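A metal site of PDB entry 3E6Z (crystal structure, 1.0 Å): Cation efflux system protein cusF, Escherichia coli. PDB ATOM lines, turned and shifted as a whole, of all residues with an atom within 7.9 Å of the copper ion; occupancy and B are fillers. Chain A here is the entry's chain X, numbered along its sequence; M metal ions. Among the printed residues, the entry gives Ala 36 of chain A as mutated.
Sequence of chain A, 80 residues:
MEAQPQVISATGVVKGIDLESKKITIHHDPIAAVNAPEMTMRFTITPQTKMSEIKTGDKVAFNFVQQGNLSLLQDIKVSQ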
ATOM      1  N   ALA A  10     -22.898   7.748  -3.850  1.00  0.00           N
ATOM      2  CA  ALA A  10     -23.932   8.481  -3.143  1.00  0.00           C
ATOM      3  C   ALA A  10     -24.398   7.723  -1.946  1.00  0.00           C
ATOM      4  O   ALA A  10     -24.100   6.578  -1.718  1.00  0.00           O
ATOM      5  CB  ALA A  10     -25.072   8.726  -4.044  1.00  0.00           C
ATOM      6  N   ILE A  26     -34.628   5.309  -4.777  1.00  0.00           N
ATOM      7  CA  ILE A  26     -33.816   5.837  -3.672  1.00  0.00           C
ATOM      8  C   ILE A  26     -33.954   7.303  -3.610  1.00  0.00           C
ATOM      9  O   ILE A  26     -33.823   8.013  -4.641  1.00  0.00           O
ATOM     10  CB  ILE A  26     -32.297   5.460  -3.830  1.00  0.00           C
ATOM     11  CG1 ILE A  26     -32.169   3.954  -3.963  1.00  0.00           C
ATOM     12  CG2 ILE A  26     -31.454   6.063  -2.654  1.00  0.00           C
ATOM     13  CD1 ILE A  26     -30.671   3.478  -4.230  1.00  0.00           C
ATOM     14  N   HIS A  28     -31.857  10.092  -2.608  1.00  0.00           N
ATOM     15  CA  HIS A  28     -30.438  10.280  -2.326  1.00  0.00           C
ATOM     16  C   HIS A  28     -30.151  11.662  -1.669  1.00  0.00           C
ATOM     17  O   HIS A  28     -30.885  12.630  -1.922  1.00  0.00           O
ATOM     18  CB  HIS A  28     -29.566  10.025  -3.590  1.00  0.00           C
ATOM     19  CG  HIS A  28     -29.680  11.066  -4.675  1.00  0.00           C
ATOM     20  ND1 HIS A  28     -29.238  12.345  -4.557  1.00  0.00           N
ATOM     21  CD2 HIS A  28     -30.058  10.973  -5.992  1.00  0.00           C
ATOM     22  CE1 HIS A  28     -29.350  13.009  -5.734  1.00  0.00           C
ATOM     23  NE2 HIS A  28     -29.855  12.187  -6.655  1.00  0.00           N
ATOM     24  N   ASP A  29     -29.161  11.605  -0.810  1.00  0.00           N
ATOM     25  CA  ASP A  29     -28.580  12.818  -0.182  1.00  0.00           C
ATOM     26  C   ASP A  29     -27.916  13.635  -1.261  1.00  0.00           C
ATOM     27  O   ASP A  29     -27.674  13.137  -2.383  1.00  0.00           O
ATOM     28  CB  ASP A  29     -27.613  12.396   0.886  1.00  0.00           C
ATOM     29  CG  ASP A  29     -28.299  11.502   1.906  1.00  0.00           C
ATOM     30  OD1 ASP A  29     -29.472  11.907   2.377  1.00  0.00           O
ATOM     31  OD2 ASP A  29     -27.696  10.542   2.331  1.00  0.00           O
ATOM     32  N   PRO A  30     -27.615  14.915  -0.992  1.00  0.00           N
ATOM     33  CA  PRO A  30     -26.904  15.697  -2.032  1.00  0.00           C
ATOM     34  C   PRO A  30     -25.633  14.952  -2.480  1.00  0.00           C
ATOM     35  O   PRO A  30     -24.929  14.311  -1.663  1.00  0.00           O
ATOM     36  CB  PRO A  30     -26.626  17.041  -1.324  1.00  0.00           C
ATOM     37  CG  PRO A  30     -27.686  17.118  -0.251  1.00  0.00           C
ATOM     38  CD  PRO A  30     -27.843  15.702   0.228  1.00  0.00           C
ATOM     39  N   ILE A  31     -25.357  15.139  -3.766  1.00  0.00           N
ATOM     40  CA  ILE A  31     -24.128  14.477  -4.326  1.00  0.00           C
ATOM     41  C   ILE A  31     -23.144  15.572  -4.816  1.00  0.00           C
ATOM     42  O   ILE A  31     -23.386  16.171  -5.887  1.00  0.00           O
ATOM     43  CB  ILE A  31     -24.427  13.561  -5.506  1.00  0.00           C
ATOM     44  CG1 ILE A  31     -25.541  12.512  -5.170  1.00  0.00           C
ATOM     45  CG2 ILE A  31     -23.094  12.798  -5.914  1.00  0.00           C
ATOM     46  CD1 ILE A  31     -25.961  11.725  -6.293  1.00  0.00           C
ATOM     47  N   VAL A  34     -21.394  15.838  -8.589  1.00  0.00           N
ATOM     48  CA  VAL A  34     -22.206  16.236  -9.684  1.00  0.00           C
ATOM     49  C   VAL A  34     -23.081  17.449  -9.363  1.00  0.00           C
ATOM     50  O   VAL A  34     -23.999  17.788 -10.106  1.00  0.00           O
ATOM     51  CB  VAL A  34     -23.050  15.078 -10.283  1.00  0.00           C
ATOM     52  CG1 VAL A  34     -22.149  14.000 -10.850  1.00  0.00           C
ATOM     53  CG2 VAL A  34     -23.998  14.499  -9.239  1.00  0.00           C
ATOM     54  N   ALA A  36     -25.528  17.803  -7.246  1.00  0.00           N
ATOM     55  CA  ALA A  36     -26.982  17.411  -7.158  1.00  0.00           C
ATOM     56  C   ALA A  36     -27.493  17.698  -5.792  1.00  0.00           C
ATOM     57  O   ALA A  36     -26.760  17.446  -4.798  1.00  0.00           O
ATOM     58  CB  ALA A  36     -27.135  15.974  -7.447  1.00  0.00           C
ATOM     59  N   PRO A  37     -28.740  18.173  -5.710  1.00  0.00           N
ATOM     60  CA  PRO A  37     -29.422  18.300  -4.411  1.00  0.00           C
ATOM     61  C   PRO A  37     -29.992  16.918  -4.056  1.00  0.00           C
ATOM     62  O   PRO A  37     -29.779  15.922  -4.781  1.00  0.00           O
ATOM     63  CB  PRO A  37     -30.562  19.218  -4.721  1.00  0.00           C
ATOM     64  CG  PRO A  37     -30.902  18.873  -6.201  1.00  0.00           C
ATOM     65  CD  PRO A  37     -29.614  18.526  -6.821  1.00  0.00           C
ATOM     66  N   GLU A  38     -30.728  16.861  -2.948  1.00  0.00           N
ATOM     67  CA  GLU A  38     -31.477  15.686  -2.611  1.00  0.00           C
ATOM     68  C   GLU A  38     -32.463  15.364  -3.773  1.00  0.00           C
ATOM     69  O   GLU A  38     -33.091  16.267  -4.341  1.00  0.00           O
ATOM     70  CB  GLU A  38     -32.277  15.889  -1.364  1.00  0.00           C
ATOM     71  CG  GLU A  38     -31.514  16.225  -0.104  1.00  0.00           C
ATOM     72  CD  GLU A  38     -31.296  17.694   0.102  1.00  0.00           C
ATOM     73  OE1 GLU A  38     -31.459  18.510  -0.878  1.00  0.00           O
ATOM     74  OE2 GLU A  38     -30.954  18.056   1.277  1.00  0.00           O
ATOM     75  N   MET A  39     -32.592  14.096  -4.169  1.00  0.00           N
ATOM     76  CA  MET A  39     -33.507  13.744  -5.238  1.00  0.00           C
ATOM     77  C   MET A  39     -34.019  12.311  -5.065  1.00  0.00           C
ATOM     78  O   MET A  39     -33.231  11.464  -4.669  1.00  0.00           O
ATOM     79  CB  MET A  39     -32.827  13.719  -6.665  1.00  0.00           C
ATOM     80  CG  MET A  39     -32.171  14.993  -7.091  1.00  0.00           C
ATOM     81  SD  MET A  39     -31.178  14.784  -8.562  1.00  0.00           S
ATOM     82  CE  MET A  39     -32.461  14.724  -9.763  1.00  0.00           C
ATOM     83  N   THR A  40     -35.279  12.024  -5.460  1.00  0.00           N
ATOM     84  CA  THR A  40     -35.735  10.635  -5.554  1.00  0.00           C
ATOM     85  C   THR A  40     -35.507  10.199  -6.995  1.00  0.00           C
ATOM     86  O   THR A  40     -36.008  10.833  -7.964  1.00  0.00           O
ATOM     87  CB  THR A  40     -37.261  10.506  -5.207  1.00  0.00           C
ATOM     88  OG1 THR A  40     -37.464  10.913  -3.842  1.00  0.00           O
ATOM     89  CG2 THR A  40     -37.791   9.126  -5.475  1.00  0.00           C
ATOM     90  N   MET A  41     -34.783   9.094  -7.171  1.00  0.00           N
ATOM     91  CA  MET A  41     -34.416   8.589  -8.487  1.00  0.00           C
ATOM     92  C   MET A  41     -34.596   7.069  -8.502  1.00  0.00           C
ATOM     93  O   MET A  41     -34.514   6.412  -7.452  1.00  0.00           O
ATOM     94  CB  MET A  41     -32.958   8.944  -8.927  1.00  0.00           C
ATOM     95  CG  MET A  41     -32.642  10.416  -8.797  1.00  0.00           C
ATOM     96  SD  MET A  41     -31.052  10.835  -9.474  1.00  0.00           S
ATOM     97  CE  MET A  41     -31.392  11.038 -11.216  1.00  0.00           C
ATOM     98  N   ARG A  42     -34.759   6.529  -9.732  1.00  0.00           N
ATOM     99  CA  ARG A  42     -34.827   5.100  -9.949  1.00  0.00           C
ATOM    100  C   ARG A  42     -33.470   4.559 -10.365  1.00  0.00           C
ATOM    101  O   ARG A  42     -32.841   5.085 -11.353  1.00  0.00           O
ATOM    102  CB  ARG A  42     -35.820   4.739 -11.069  1.00  0.00           C
ATOM    103  CG  ARG A  42     -37.246   5.050 -10.691  1.00  0.00           C
ATOM    104  CD  ARG A  42     -38.172   5.157 -11.918  1.00  0.00           C
ATOM    105  NE  ARG A  42     -38.309   3.969 -12.765  1.00  0.00           N
ATOM    106  CZ  ARG A  42     -39.111   2.933 -12.515  1.00  0.00           C
ATOM    107  NH1 ARG A  42     -39.160   1.908 -13.358  1.00  0.00           N
ATOM    108  NH2 ARG A  42     -39.822   2.817 -11.400  1.00  0.00           N
ATOM    109  N   PHE A  43     -32.998   3.535  -9.703  1.00  0.00           N
ATOM    110  CA  PHE A  43     -31.686   2.884  -9.978  1.00  0.00           C
ATOM    111  C   PHE A  43     -31.944   1.466 -10.365  1.00  0.00           C
ATOM    112  O   PHE A  43     -32.841   0.772  -9.895  1.00  0.00           O
ATOM    113  CB  PHE A  43     -30.796   2.964  -8.716  1.00  0.00           C
ATOM    114  CG  PHE A  43     -30.443   4.376  -8.345  1.00  0.00           C
ATOM    115  CD1 PHE A  43     -29.304   4.988  -8.958  1.00  0.00           C
ATOM    116  CD2 PHE A  43     -31.281   5.178  -7.491  1.00  0.00           C
ATOM    117  CE1 PHE A  43     -29.036   6.297  -8.817  1.00  0.00           C
ATOM    118  CE2 PHE A  43     -30.937   6.497  -7.288  1.00  0.00           C
ATOM    119  CZ  PHE A  43     -29.853   7.094  -7.908  1.00  0.00           C
ATOM    120  N   PHE A  62     -24.129   3.668  -2.122  1.00  0.00           N
ATOM    121  CA  PHE A  62     -24.238   2.978  -3.366  1.00  0.00           C
ATOM    122  C   PHE A  62     -23.440   3.757  -4.363  1.00  0.00           C
ATOM    123  O   PHE A  62     -23.080   4.903  -4.239  1.00  0.00           O
ATOM    124  CB  PHE A  62     -25.731   2.768  -3.810  1.00  0.00           C
ATOM    125  CG  PHE A  62     -26.475   4.042  -3.980  1.00  0.00           C
ATOM    126  CD1 PHE A  62     -27.009   4.801  -2.875  1.00  0.00           C
ATOM    127  CD2 PHE A  62     -26.751   4.564  -5.305  1.00  0.00           C
ATOM    128  CE1 PHE A  62     -27.695   5.954  -3.101  1.00  0.00           C
ATOM    129  CE2 PHE A  62     -27.475   5.676  -5.493  1.00  0.00           C
ATOM    130  CZ  PHE A  62     -28.004   6.403  -4.406  1.00  0.00           C
ATOM    131  N   PHE A  64     -23.068   4.131  -8.793  1.00  0.00           N
ATOM    132  CA  PHE A  64     -23.804   3.818 -10.050  1.00  0.00           C
ATOM    133  C   PHE A  64     -23.090   4.547 -11.198  1.00  0.00           C
ATOM    134  O   PHE A  64     -22.273   5.427 -11.053  1.00  0.00           O
ATOM    135  CB  PHE A  64     -25.297   4.313  -9.904  1.00  0.00           C
ATOM    136  CG  PHE A  64     -25.446   5.815  -9.714  1.00  0.00           C
ATOM    137  CD1 PHE A  64     -25.346   6.362  -8.412  1.00  0.00           C
ATOM    138  CD2 PHE A  64     -25.675   6.691 -10.767  1.00  0.00           C
ATOM    139  CE1 PHE A  64     -25.555   7.716  -8.182  1.00  0.00           C
ATOM    140  CE2 PHE A  64     -25.859   8.037 -10.513  1.00  0.00           C
ATOM    141  CZ  PHE A  64     -25.801   8.524  -9.245  1.00  0.00           C
ATOM    142  N   GLN A  66     -24.060   6.209 -15.087  1.00  0.00           N
ATOM    143  CA  GLN A  66     -25.212   6.687 -15.963  1.00  0.00           C
ATOM    144  C   GLN A  66     -25.019   6.126 -17.342  1.00  0.00           C
ATOM    145  O   GLN A  66     -23.878   6.103 -17.920  1.00  0.00           O
ATOM    146  CB  GLN A  66     -25.238   8.224 -16.010  1.00  0.00           C
ATOM    147  CG  GLN A  66     -26.563   8.777 -16.470  1.00  0.00           C
ATOM    148  CD  GLN A  66     -27.700   8.470 -15.468  1.00  0.00           C
ATOM    149  OE1 GLN A  66     -27.502   8.281 -14.244  1.00  0.00           O
ATOM    150  NE2 GLN A  66     -28.943   8.520 -16.021  1.00  0.00           N
ATOM    151  N   SER A  71     -29.646   4.722 -14.512  1.00  0.00           N
ATOM    152  CA  SER A  71     -28.554   4.794 -13.534  1.00  0.00           C
ATOM    153  C   SER A  71     -28.328   3.350 -13.067  1.00  0.00           C
ATOM    154  O   SER A  71     -29.168   2.788 -12.332  1.00  0.00           O
ATOM    155  CB  SER A  71     -28.965   5.726 -12.359  1.00  0.00           C
ATOM    156  OG  SER A  71     -29.259   7.003 -12.766  1.00  0.00           O
HETATM  157 CU    CU M   1     -30.144  12.749  -8.531  1.00  0.00          CU
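The copper ion is bound by NE2 of His 28 (2.0 Å).
The copper ion is bound by the side-chain sulfur (SD) of Met 39 (2.3 Å).
SD of Met 41 binds the copper ion (2.3 Å).
The copper ion has three donor atoms within binding distance.
Of the 19 residues printed, 3 come within 4 Å of the copper ion.
The nearest printed residue that does not touch the copper ion is Ala 36 (4.5 Å).
The backbone NH (N) of Ile 26 sits at hydrogen-bond distance from the backbone carbonyl oxygen (O) of Met 41 (2.9 Å).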
